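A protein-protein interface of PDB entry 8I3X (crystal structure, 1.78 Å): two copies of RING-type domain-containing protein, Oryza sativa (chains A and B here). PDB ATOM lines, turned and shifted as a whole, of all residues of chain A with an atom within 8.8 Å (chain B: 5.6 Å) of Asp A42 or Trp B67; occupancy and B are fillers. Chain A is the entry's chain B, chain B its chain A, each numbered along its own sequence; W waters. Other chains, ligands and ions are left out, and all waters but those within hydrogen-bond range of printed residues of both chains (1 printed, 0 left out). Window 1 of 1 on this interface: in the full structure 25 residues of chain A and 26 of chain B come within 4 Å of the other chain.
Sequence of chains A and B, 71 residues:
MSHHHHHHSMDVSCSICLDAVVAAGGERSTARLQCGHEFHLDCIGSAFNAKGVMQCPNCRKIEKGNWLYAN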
ATOM      1  N   CYS A  14      32.335  -9.011  39.711  1.00  0.00           N
ATOM      2  CA  CYS A  14      32.116  -9.197  38.282  1.00  0.00           C
ATOM      3  C   CYS A  14      33.464  -9.272  37.577  1.00  0.00           C
ATOM      4  O   CYS A  14      34.237  -8.310  37.608  1.00  0.00           O
ATOM      5  CB  CYS A  14      31.273  -8.047  37.734  1.00  0.00           C
ATOM      6  SG  CYS A  14      31.002  -8.048  35.935  1.00  0.00           S
ATOM      7  N   ILE A  16      34.117  -8.982  34.628  1.00  0.00           N
ATOM      8  CA  ILE A  16      34.189  -8.146  33.437  1.00  0.00           C
ATOM      9  C   ILE A  16      34.702  -6.754  33.782  1.00  0.00           C
ATOM     10  O   ILE A  16      35.603  -6.222  33.122  1.00  0.00           O
ATOM     11  CB  ILE A  16      32.814  -8.098  32.749  1.00  0.00           C
ATOM     12  CG1 ILE A  16      32.447  -9.494  32.240  1.00  0.00           C
ATOM     13  CG2 ILE A  16      32.817  -7.079  31.629  1.00  0.00           C
ATOM     14  CD1 ILE A  16      31.115  -9.579  31.555  1.00  0.00           C
ATOM     15  N   CYS A  17      34.138  -6.140  34.811  1.00  0.00           N
ATOM     16  CA  CYS A  17      34.534  -4.808  35.230  1.00  0.00           C
ATOM     17  C   CYS A  17      35.299  -4.817  36.543  1.00  0.00           C
ATOM     18  O   CYS A  17      35.773  -3.760  36.977  1.00  0.00           O
ATOM     19  CB  CYS A  17      33.297  -3.914  35.352  1.00  0.00           C
ATOM     20  SG  CYS A  17      32.221  -4.335  36.744  1.00  0.00           S
ATOM     21  N   GLU A  27      21.197  -0.233  43.395  1.00  0.00           N
ATOM     22  CA  GLU A  27      22.323   0.242  42.589  1.00  0.00           C
ATOM     23  C   GLU A  27      22.316  -0.227  41.124  1.00  0.00           C
ATOM     24  O   GLU A  27      21.688   0.419  40.280  1.00  0.00           O
ATOM     25  CB  GLU A  27      23.623  -0.124  43.338  1.00  0.00           C
ATOM     26  CG  GLU A  27      24.047  -1.602  43.375  1.00  0.00           C
ATOM     27  CD  GLU A  27      23.033  -2.530  44.030  1.00  0.00           C
ATOM     28  OE1 GLU A  27      21.881  -2.126  44.290  1.00  0.00           O
ATOM     29  OE2 GLU A  27      23.377  -3.704  44.244  1.00  0.00           O
ATOM     30  N   ARG A  28      23.025  -1.306  40.797  1.00  0.00           N
ATOM     31  CA  ARG A  28      23.181  -1.792  39.434  1.00  0.00           C
ATOM     32  C   ARG A  28      22.475  -3.131  39.308  1.00  0.00           C
ATOM     33  O   ARG A  28      22.505  -3.945  40.236  1.00  0.00           O
ATOM     34  CB  ARG A  28      24.662  -1.973  39.059  1.00  0.00           C
ATOM     35  CG  ARG A  28      25.441  -0.692  38.809  1.00  0.00           C
ATOM     36  CD  ARG A  28      26.916  -1.017  38.558  1.00  0.00           C
ATOM     37  NE  ARG A  28      27.137  -1.573  37.223  1.00  0.00           N
ATOM     38  CZ  ARG A  28      28.308  -2.021  36.779  1.00  0.00           C
ATOM     39  NH1 ARG A  28      29.375  -1.977  37.561  1.00  0.00           N
ATOM     40  NH2 ARG A  28      28.411  -2.508  35.547  1.00  0.00           N
ATOM     41  N   SER A  29      21.858  -3.364  38.155  1.00  0.00           N
ATOM     42  CA  SER A  29      21.189  -4.632  37.918  1.00  0.00           C
ATOM     43  C   SER A  29      22.213  -5.753  37.834  1.00  0.00           C
ATOM     44  O   SER A  29      23.378  -5.540  37.483  1.00  0.00           O
ATOM     45  CB  SER A  29      20.365  -4.568  36.632  1.00  0.00           C
ATOM     46  OG  SER A  29      19.376  -3.559  36.740  1.00  0.00           O
ATOM     47  N   THR A  30      21.771  -6.959  38.163  1.00  0.00           N
ATOM     48  CA  THR A  30      22.673  -8.093  38.247  1.00  0.00           C
ATOM     49  C   THR A  30      22.121  -9.268  37.453  1.00  0.00           C
ATOM     50  O   THR A  30      20.931  -9.327  37.129  1.00  0.00           O
ATOM     51  CB  THR A  30      22.899  -8.512  39.699  1.00  0.00           C
ATOM     52  OG1 THR A  30      21.651  -8.935  40.258  1.00  0.00           O
ATOM     53  CG2 THR A  30      23.425  -7.332  40.504  1.00  0.00           C
ATOM     54  N   ALA A  31      23.004 -10.219  37.168  1.00  0.00           N
ATOM     55  CA  ALA A  31      22.631 -11.445  36.487  1.00  0.00           C
ATOM     56  C   ALA A  31      23.363 -12.610  37.127  1.00  0.00           C
ATOM     57  O   ALA A  31      24.474 -12.461  37.640  1.00  0.00           O
ATOM     58  CB  ALA A  31      22.959 -11.395  34.994  1.00  0.00           C
ATOM     59  N   PHE A  39      27.384 -11.504  37.469  1.00  0.00           N
ATOM     60  CA  PHE A  39      27.862 -10.354  36.727  1.00  0.00           C
ATOM     61  C   PHE A  39      26.878  -9.216  36.927  1.00  0.00           C
ATOM     62  O   PHE A  39      25.731  -9.430  37.317  1.00  0.00           O
ATOM     63  CB  PHE A  39      27.987 -10.664  35.231  1.00  0.00           C
ATOM     64  CG  PHE A  39      28.839 -11.863  34.928  1.00  0.00           C
ATOM     65  CD1 PHE A  39      30.209 -11.734  34.774  1.00  0.00           C
ATOM     66  CD2 PHE A  39      28.270 -13.117  34.792  1.00  0.00           C
ATOM     67  CE1 PHE A  39      30.998 -12.835  34.489  1.00  0.00           C
ATOM     68  CE2 PHE A  39      29.056 -14.220  34.520  1.00  0.00           C
ATOM     69  CZ  PHE A  39      30.421 -14.074  34.361  1.00  0.00           C
ATOM     70  N   HIS A  40      27.328  -8.004  36.638  1.00  0.00           N
ATOM     71  CA  HIS A  40      26.371  -6.930  36.420  1.00  0.00           C
ATOM     72  C   HIS A  40      25.636  -7.181  35.115  1.00  0.00           C
ATOM     73  O   HIS A  40      26.195  -7.733  34.165  1.00  0.00           O
ATOM     74  CB  HIS A  40      27.074  -5.578  36.378  1.00  0.00           C
ATOM     75  CG  HIS A  40      27.863  -5.288  37.613  1.00  0.00           C
ATOM     76  ND1 HIS A  40      29.234  -5.416  37.669  1.00  0.00           N
ATOM     77  CD2 HIS A  40      27.467  -4.920  38.854  1.00  0.00           C
ATOM     78  CE1 HIS A  40      29.651  -5.121  38.886  1.00  0.00           C
ATOM     79  NE2 HIS A  40      28.599  -4.820  39.625  1.00  0.00           N
ATOM     80  N   LEU A  41      24.366  -6.773  35.070  1.00  0.00           N
ATOM     81  CA  LEU A  41      23.561  -7.037  33.879  1.00  0.00           C
ATOM     82  C   LEU A  41      24.167  -6.397  32.627  1.00  0.00           C
ATOM     83  O   LEU A  41      24.252  -7.043  31.581  1.00  0.00           O
ATOM     84  CB  LEU A  41      22.125  -6.560  34.082  1.00  0.00           C
ATOM     85  CG  LEU A  41      21.202  -6.874  32.902  1.00  0.00           C
ATOM     86  CD1 LEU A  41      21.281  -8.334  32.525  1.00  0.00           C
ATOM     87  CD2 LEU A  41      19.775  -6.498  33.285  1.00  0.00           C
ATOM     88  N   ASP A  42      24.580  -5.126  32.700  1.00  0.00           N
ATOM     89  CA  ASP A  42      25.062  -4.498  31.469  1.00  0.00           C
ATOM     90  C   ASP A  42      26.406  -5.073  31.042  1.00  0.00           C
ATOM     91  O   ASP A  42      26.689  -5.164  29.841  1.00  0.00           O
ATOM     92  CB  ASP A  42      25.111  -2.963  31.611  1.00  0.00           C
ATOM     93  CG  ASP A  42      25.970  -2.480  32.773  1.00  0.00           C
ATOM     94  OD1 ASP A  42      26.516  -3.303  33.530  1.00  0.00           O
ATOM     95  OD2 ASP A  42      26.094  -1.242  32.919  1.00  0.00           O
ATOM     96  N   CYS A  43      27.235  -5.501  31.993  1.00  0.00           N
ATOM     97  CA  CYS A  43      28.493  -6.149  31.640  1.00  0.00           C
ATOM     98  C   CYS A  43      28.252  -7.422  30.837  1.00  0.00           C
ATOM     99  O   CYS A  43      28.762  -7.574  29.720  1.00  0.00           O
ATOM    100  CB  CYS A  43      29.286  -6.466  32.899  1.00  0.00           C
ATOM    101  SG  CYS A  43      29.909  -5.000  33.679  1.00  0.00           S
ATOM    102  N   ILE A  44      27.503  -8.366  31.409  1.00  0.00           N
ATOM    103  CA  ILE A  44      27.345  -9.663  30.756  1.00  0.00           C
ATOM    104  C   ILE A  44      26.488  -9.536  29.502  1.00  0.00           C
ATOM    105  O   ILE A  44      26.719 -10.236  28.512  1.00  0.00           O
ATOM    106  CB  ILE A  44      26.775 -10.702  31.749  1.00  0.00           C
ATOM    107  CG1 ILE A  44      26.933 -12.121  31.200  1.00  0.00           C
ATOM    108  CG2 ILE A  44      25.328 -10.426  32.061  1.00  0.00           C
ATOM    109  CD1 ILE A  44      28.368 -12.563  31.083  1.00  0.00           C
ATOM    110  N   GLY A  45      25.493  -8.642  29.516  1.00  0.00           N
ATOM    111  CA  GLY A  45      24.669  -8.455  28.329  1.00  0.00           C
ATOM    112  C   GLY A  45      25.471  -7.918  27.162  1.00  0.00           C
ATOM    113  O   GLY A  45      25.304  -8.356  26.019  1.00  0.00           O
ATOM    114  N   SER A  46      26.360  -6.963  27.429  1.00  0.00           N
ATOM    115  CA  SER A  46      27.227  -6.470  26.363  1.00  0.00           C
ATOM    116  C   SER A  46      28.182  -7.549  25.882  1.00  0.00           C
ATOM    117  O   SER A  46      28.510  -7.606  24.689  1.00  0.00           O
ATOM    118  CB  SER A  46      28.005  -5.250  26.845  1.00  0.00           C
ATOM    119  OG  SER A  46      27.112  -4.229  27.233  1.00  0.00           O
ATOM    120  N   ALA A  47      28.616  -8.431  26.786  1.00  0.00           N
ATOM    121  CA  ALA A  47      29.523  -9.505  26.388  1.00  0.00           C
ATOM    122  C   ALA A  47      28.811 -10.523  25.501  1.00  0.00           C
ATOM    123  O   ALA A  47      29.363 -10.977  24.489  1.00  0.00           O
ATOM    124  CB  ALA A  47      30.104 -10.184  27.631  1.00  0.00           C
ATOM    125  N   PHE A  48      27.597 -10.921  25.892  1.00  0.00           N
ATOM    126  CA  PHE A  48      26.781 -11.773  25.034  1.00  0.00           C
ATOM    127  C   PHE A  48      26.545 -11.122  23.668  1.00  0.00           C
ATOM    128  O   PHE A  48      26.652 -11.786  22.632  1.00  0.00           O
ATOM    129  CB  PHE A  48      25.449 -12.091  25.722  1.00  0.00           C
ATOM    130  CG  PHE A  48      25.564 -13.058  26.877  1.00  0.00           C
ATOM    131  CD1 PHE A  48      26.783 -13.599  27.250  1.00  0.00           C
ATOM    132  CD2 PHE A  48      24.436 -13.410  27.606  1.00  0.00           C
ATOM    133  CE1 PHE A  48      26.871 -14.484  28.321  1.00  0.00           C
ATOM    134  CE2 PHE A  48      24.529 -14.295  28.662  1.00  0.00           C
ATOM    135  CZ  PHE A  48      25.741 -14.820  29.022  1.00  0.00           C
ATOM    136  N   ASN A  49      26.247  -9.817  23.646  1.00  0.00           N
ATOM    137  CA  ASN A  49      25.974  -9.138  22.381  1.00  0.00           C
ATOM    138  C   ASN A  49      27.183  -9.165  21.456  1.00  0.00           C
ATOM    139  O   ASN A  49      27.039  -9.289  20.234  1.00  0.00           O
ATOM    140  CB  ASN A  49      25.559  -7.690  22.637  1.00  0.00           C
ATOM    141  CG  ASN A  49      24.156  -7.572  23.165  1.00  0.00           C
ATOM    142  OD1 ASN A  49      23.377  -8.527  23.106  1.00  0.00           O
ATOM    143  ND2 ASN A  49      23.821  -6.399  23.695  1.00  0.00           N
ATOM    144  N   TRP A  67      18.912 -15.767  22.974  1.00  0.00           N
ATOM    145  CA  TRP A  67      19.468 -14.418  23.047  1.00  0.00           C
ATOM    146  C   TRP A  67      19.211 -13.719  21.718  1.00  0.00           C
ATOM    147  O   TRP A  67      19.826 -14.053  20.696  1.00  0.00           O
ATOM    148  CB  TRP A  67      20.956 -14.467  23.375  1.00  0.00           C
ATOM    149  CG  TRP A  67      21.544 -13.117  23.651  1.00  0.00           C
ATOM    150  CD1 TRP A  67      22.279 -12.336  22.787  1.00  0.00           C
ATOM    151  CD2 TRP A  67      21.463 -12.388  24.877  1.00  0.00           C
ATOM    152  NE1 TRP A  67      22.647 -11.163  23.411  1.00  0.00           N
ATOM    153  CE2 TRP A  67      22.153 -11.167  24.690  1.00  0.00           C
ATOM    154  CE3 TRP A  67      20.853 -12.637  26.110  1.00  0.00           C
ATOM    155  CZ2 TRP A  67      22.268 -10.217  25.691  1.00  0.00           C
ATOM    156  CZ3 TRP A  67      20.968 -11.680  27.110  1.00  0.00           C
ATOM    157  CH2 TRP A  67      21.666 -10.490  26.895  1.00  0.00           C
ATOM    158  N   LEU A  68      18.293 -12.762  21.727  1.00  0.00           N
ATOM    159  CA  LEU A  68      17.866 -12.082  20.517  1.00  0.00           C
ATOM    160  C   LEU A  68      18.330 -10.636  20.555  1.00  0.00           C
ATOM    161  O   LEU A  68      18.527 -10.058  21.626  1.00  0.00           O
ATOM    162  CB  LEU A  68      16.348 -12.125  20.360  1.00  0.00           C
ATOM    163  CG  LEU A  68      15.689 -13.498  20.415  1.00  0.00           C
ATOM    164  CD1 LEU A  68      14.188 -13.333  20.502  1.00  0.00           C
ATOM    165  CD2 LEU A  68      16.071 -14.276  19.182  1.00  0.00           C
ATOM    166  N   TYR A  69      18.518 -10.059  19.371  1.00  0.00           N
ATOM    167  CA  TYR A  69      18.894  -8.655  19.303  1.00  0.00           C
ATOM    168  C   TYR A  69      17.693  -7.725  19.150  1.00  0.00           C
ATOM    169  O   TYR A  69      17.840  -6.518  19.341  1.00  0.00           O
ATOM    170  CB  TYR A  69      19.886  -8.430  18.161  1.00  0.00           C
ATOM    171  CG  TYR A  69      21.245  -9.019  18.451  1.00  0.00           C
ATOM    172  CD1 TYR A  69      21.512 -10.368  18.213  1.00  0.00           C
ATOM    173  CD2 TYR A  69      22.264  -8.233  18.962  1.00  0.00           C
ATOM    174  CE1 TYR A  69      22.768 -10.911  18.481  1.00  0.00           C
ATOM    175  CE2 TYR A  69      23.516  -8.764  19.236  1.00  0.00           C
ATOM    176  CZ  TYR A  69      23.758 -10.102  18.993  1.00  0.00           C
ATOM    177  OH  TYR A  69      25.000 -10.621  19.272  1.00  0.00           O
ATOM    178  N   ILE B  44      15.037 -10.632  29.342  1.00  0.00           N
ATOM    179  CA  ILE B  44      15.229  -9.200  29.541  1.00  0.00           C
ATOM    180  C   ILE B  44      16.352  -8.688  28.652  1.00  0.00           C
ATOM    181  O   ILE B  44      16.301  -7.542  28.198  1.00  0.00           O
ATOM    182  CB  ILE B  44      15.479  -8.849  31.018  1.00  0.00           C
ATOM    183  CG1 ILE B  44      15.339  -7.338  31.236  1.00  0.00           C
ATOM    184  CG2 ILE B  44      16.839  -9.343  31.483  1.00  0.00           C
ATOM    185  CD1 ILE B  44      13.895  -6.813  31.067  1.00  0.00           C
ATOM    186  N   GLY B  45      17.360  -9.523  28.380  1.00  0.00           N
ATOM    187  CA  GLY B  45      18.405  -9.123  27.449  1.00  0.00           C
ATOM    188  C   GLY B  45      17.846  -8.785  26.083  1.00  0.00           C
ATOM    189  O   GLY B  45      18.168  -7.741  25.506  1.00  0.00           O
ATOM    190  N   SER B  46      16.968  -9.646  25.560  1.00  0.00           N
ATOM    191  CA  SER B  46      16.409  -9.403  24.231  1.00  0.00           C
ATOM    192  C   SER B  46      15.525  -8.166  24.227  1.00  0.00           C
ATOM    193  O   SER B  46      15.447  -7.455  23.221  1.00  0.00           O
ATOM    194  CB  SER B  46      15.625 -10.627  23.764  1.00  0.00           C
ATOM    195  OG  SER B  46      16.423 -11.801  23.900  1.00  0.00           O
ATOM    196  N   PHE B  48      15.881  -5.399  26.218  1.00  0.00           N
ATOM    197  CA  PHE B  48      16.770  -4.238  26.200  1.00  0.00           C
ATOM    198  C   PHE B  48      17.392  -4.064  24.825  1.00  0.00           C
ATOM    199  O   PHE B  48      17.550  -2.937  24.344  1.00  0.00           O
ATOM    200  CB  PHE B  48      17.889  -4.393  27.236  1.00  0.00           C
ATOM    201  CG  PHE B  48      17.445  -4.215  28.664  1.00  0.00           C
ATOM    202  CD1 PHE B  48      16.127  -3.926  28.983  1.00  0.00           C
ATOM    203  CD2 PHE B  48      18.371  -4.339  29.686  1.00  0.00           C
ATOM    204  CE1 PHE B  48      15.737  -3.773  30.324  1.00  0.00           C
ATOM    205  CE2 PHE B  48      17.989  -4.195  31.018  1.00  0.00           C
ATOM    206  CZ  PHE B  48      16.677  -3.907  31.327  1.00  0.00           C
ATOM    207  N   ASN B  49      17.739  -5.180  24.175  1.00  0.00           N
ATOM    208  CA  ASN B  49      18.379  -5.117  22.860  1.00  0.00           C
ATOM    209  C   ASN B  49      17.476  -4.482  21.813  1.00  0.00           C
ATOM    210  O   ASN B  49      17.967  -3.866  20.852  1.00  0.00           O
ATOM    211  CB  ASN B  49      18.781  -6.522  22.403  1.00  0.00           C
ATOM    212  CG  ASN B  49      20.107  -6.968  22.972  1.00  0.00           C
ATOM    213  OD1 ASN B  49      20.848  -6.172  23.548  1.00  0.00           O
ATOM    214  ND2 ASN B  49      20.430  -8.246  22.793  1.00  0.00           N
ATOM    215  N   GLY B  52      17.755  -0.538  23.133  1.00  0.00           N
ATOM    216  CA  GLY B  52      18.995   0.121  23.487  1.00  0.00           C
ATOM    217  C   GLY B  52      18.970   0.803  24.832  1.00  0.00           C
ATOM    218  O   GLY B  52      19.875   1.591  25.134  1.00  0.00           O
ATOM    219  N   VAL B  53      17.954   0.522  25.649  1.00  0.00           N
ATOM    220  CA  VAL B  53      17.746   1.186  26.929  1.00  0.00           C
ATOM    221  C   VAL B  53      17.452   0.123  27.979  1.00  0.00           C
ATOM    222  O   VAL B  53      16.708  -0.824  27.713  1.00  0.00           O
ATOM    223  CB  VAL B  53      16.574   2.185  26.860  1.00  0.00           C
ATOM    224  CG1 VAL B  53      16.323   2.823  28.220  1.00  0.00           C
ATOM    225  CG2 VAL B  53      16.823   3.239  25.825  1.00  0.00           C
ATOM    226  N   MET B  54      18.016   0.296  29.176  1.00  0.00           N
ATOM    227  CA  MET B  54      17.755  -0.631  30.286  1.00  0.00           C
ATOM    228  C   MET B  54      16.520  -0.168  31.056  1.00  0.00           C
ATOM    229  O   MET B  54      16.595   0.302  32.193  1.00  0.00           O
ATOM    230  CB  MET B  54      18.967  -0.721  31.207  1.00  0.00           C
ATOM    231  CG  MET B  54      20.235  -1.203  30.515  1.00  0.00           C
ATOM    232  SD  MET B  54      21.711  -1.261  31.553  1.00  0.00           S
ATOM    233  CE  MET B  54      21.361  -2.706  32.557  1.00  0.00           C
ATOM    234  N   GLY B  65      22.757   2.444  32.815  1.00  0.00           N
ATOM    235  CA  GLY B  65      23.902   1.581  32.621  1.00  0.00           C
ATOM    236  C   GLY B  65      24.508   1.763  31.241  1.00  0.00           C
ATOM    237  O   GLY B  65      24.188   2.695  30.502  1.00  0.00           O
ATOM    238  N   ASN B  66      25.410   0.851  30.897  1.00  0.00           N
ATOM    239  CA  ASN B  66      26.143   0.889  29.628  1.00  0.00           C
ATOM    240  C   ASN B  66      25.751  -0.359  28.843  1.00  0.00           C
ATOM    241  O   ASN B  66      26.428  -1.386  28.914  1.00  0.00           O
ATOM    242  CB  ASN B  66      27.645   0.960  29.868  1.00  0.00           C
ATOM    243  CG  ASN B  66      28.076   2.299  30.431  1.00  0.00           C
ATOM    244  OD1 ASN B  66      28.418   2.412  31.608  1.00  0.00           O
ATOM    245  ND2 ASN B  66      28.055   3.327  29.593  1.00  0.00           N
ATOM    246  N   TRP B  67      24.648  -0.275  28.108  1.00  0.00           N
ATOM    247  CA  TRP B  67      24.120  -1.424  27.373  1.00  0.00           C
ATOM    248  C   TRP B  67      24.660  -1.353  25.953  1.00  0.00           C
ATOM    249  O   TRP B  67      24.154  -0.592  25.124  1.00  0.00           O
ATOM    250  CB  TRP B  67      22.598  -1.431  27.376  1.00  0.00           C
ATOM    251  CG  TRP B  67      22.040  -2.710  26.839  1.00  0.00           C
ATOM    252  CD1 TRP B  67      21.560  -2.938  25.570  1.00  0.00           C
ATOM    253  CD2 TRP B  67      21.931  -3.950  27.537  1.00  0.00           C
ATOM    254  NE1 TRP B  67      21.149  -4.243  25.450  1.00  0.00           N
ATOM    255  CE2 TRP B  67      21.357  -4.884  26.645  1.00  0.00           C
ATOM    256  CE3 TRP B  67      22.247  -4.361  28.840  1.00  0.00           C
ATOM    257  CZ2 TRP B  67      21.105  -6.205  27.011  1.00  0.00           C
ATOM    258  CZ3 TRP B  67      21.991  -5.668  29.208  1.00  0.00           C
ATOM    259  CH2 TRP B  67      21.424  -6.581  28.296  1.00  0.00           C
ATOM    260  N   LEU B  68      25.687  -2.143  25.669  1.00  0.00           N
ATOM    261  CA  LEU B  68      26.420  -2.044  24.414  1.00  0.00           C
ATOM    262  C   LEU B  68      26.148  -3.258  23.542  1.00  0.00           C
ATOM    263  O   LEU B  68      25.897  -4.352  24.044  1.00  0.00           O
ATOM    264  CB  LEU B  68      27.922  -1.926  24.655  1.00  0.00           C
ATOM    265  CG  LEU B  68      28.386  -0.851  25.630  1.00  0.00           C
ATOM    266  CD1 LEU B  68      29.875  -0.990  25.929  1.00  0.00           C
ATOM    267  CD2 LEU B  68      28.072   0.521  25.063  1.00  0.00           C
ATOM    268  N   TYR B  69      26.246  -3.070  22.225  1.00  0.00           N
ATOM    269  CA  TYR B  69      25.988  -4.167  21.302  1.00  0.00           C
ATOM    270  C   TYR B  69      27.264  -4.820  20.786  1.00  0.00           C
ATOM    271  O   TYR B  69      27.180  -5.801  20.046  1.00  0.00           O
ATOM    272  CB  TYR B  69      25.142  -3.698  20.113  1.00  0.00           C
ATOM    273  CG  TYR B  69      23.728  -3.228  20.436  1.00  0.00           C
ATOM    274  CD1 TYR B  69      23.473  -1.898  20.746  1.00  0.00           C
ATOM    275  CD2 TYR B  69      22.647  -4.106  20.393  1.00  0.00           C
ATOM    276  CE1 TYR B  69      22.176  -1.452  21.031  1.00  0.00           C
ATOM    277  CE2 TYR B  69      21.354  -3.672  20.658  1.00  0.00           C
ATOM    278  CZ  TYR B  69      21.122  -2.350  20.982  1.00  0.00           C
ATOM    279  OH  TYR B  69      19.836  -1.910  21.244  1.00  0.00           O
HETATM  280  O   HOH W   1      29.102  -2.289  29.201  1.00  0.00           O
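Water W1 lies within hydrogen-bond range of the backbone carbonyl oxygen of Asn B66 (2.8 Å) and the side-chain hydroxyl of Ser A46 (3.4 Å).
Printed residues of chain A within 4 Å of Trp B67: Leu A41 (3.6 Å), Asp A42 (3.9 Å), Gly A45 (3.7 Å), Ser A46 (3.99 Å) and Asn A49 (3.9 Å). Of the printed residues of chain A, Ser B46 touches Leu A68 (3.0 Å). Of the printed residues of chain B, Ser A46 touches Asn B66 (3.4 Å), Trp B67 (3.99 Å) and Leu B68 (3.0 Å). Printed residues of chain B within 4 Å of Tyr A69: Asn B49. Ala A31 touches none of the printed residues of chain B. Phe A39 touches none of the printed residues of chain B. The nearest residue of chain B that does not touch Asp A42 is Leu B68 (5.2 Å). The nearest printed residue of chain A that does not touch Trp B67 is Trp A67 (4.2 Å). The nearest printed residue of chain B that does not touch Trp A67 is Ser B46 (4.03 Å).
The side-chain amide oxygen of Asn B49 is in hydrogen-bond range of the indole nitrogen of Trp B67, 2.7 Å away. OH of Tyr B69 is in hydrogen-bond range of O of Asn B49 (2.7 Å). N of Gly B52 lies within hydrogen-bond range of OH of Tyr B69, 3.1 Å away. O of Asp A42 is in hydrogen-bond range of OG of Ser A46, at 2.8 Å. OD1 of Asn A49 sits at hydrogen-bond distance from NE1 of Trp A67, at 2.8 Å. The backbone carbonyl oxygen (O) of Asn A49 sits at hydrogen-bond distance from the side-chain hydroxyl (OH) of Tyr A69 (2.6 Å).
Among the printed residues, pairs that only touch across the chains: Leu A41 with Trp B67 (3.6 Å), Trp A67 with Gly B45 (3.6 Å), Asp A42 with Gly B65 (3.6 Å), Leu A41 with Phe B48 (3.7 Å), Trp A67 with Asn B49 (3.7 Å), Gly A45 with Trp B67 (3.7 Å), Asp A42 with Met B54 (3.8 Å), Asp A42 with Trp B67 (3.9 Å), Asn A49 with Trp B67 (3.9 Å) and Ser A46 with Trp B67 (3.99 Å).
N of Leu A68 is in hydrogen-bond range of OG of Ser B46. The side-chain amide nitrogen (ND2) of Asn B49 lies within hydrogen-bond range of the side-chain amide oxygen (OD1) of Asn A49 (3.0 Å). The side-chain amide nitrogen of Asn B49 is in hydrogen-bond range of the backbone carbonyl oxygen of Leu A68, 2.9 Å away. The backbone NH (N) of Asn B66 lies within hydrogen-bond range of the side-chain carboxylate (OD2) of Asp A42, at 3.0 Å. The backbone carbonyl oxygen (O) of Asn B66 sits at hydrogen-bond distance from the side-chain hydroxyl (OG) of Ser A46 (3.4 Å). N of Leu B68 lies within hydrogen-bond range of OG of Ser A46 (3.0 Å). The backbone carbonyl oxygen of Leu B68 sits at hydrogen-bond distance from the side-chain amide nitrogen of Asn A49 (2.9 Å). The backbone carbonyl oxygen (O) of Asn A49 lies close to the backbone carbonyl oxygen (O) of Tyr B69. O of Tyr A69 sits close to O of Asn B49 (3.1 Å).
Gly A45 touches Trp B67, and with the chains exchanged Trp A67 touches Gly B45. Ser A46 touches Trp B67, but with the chains exchanged Trp A67 does not touch Ser B46 (4.03 Å). Asn B49 touches its own counterpart, Asn A49. Asn A49 touches Trp B67, and with the chains exchanged Trp A67 touches Asn B49. Positions printed for both chains: 44, 45, 46, 48, 49, 67, 68 and 69.
Of the 22 printed residues of chain A, 8 touch a printed residue of chain B. Of the 13 printed residues of chain B, 10 touch a printed residue of chain A. Printed residues of chain B that touch a printed residue of chain A: Gly B45, Ser B46, Phe B48, Asn B49, Met B54, Gly B65, Asn B66, Trp B67, Leu B68 and Tyr B69. Among the printed residues, no Asp or Glu carboxylate lies within 4 Å of a Lys or Arg side-chain nitrogen of the other chain.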
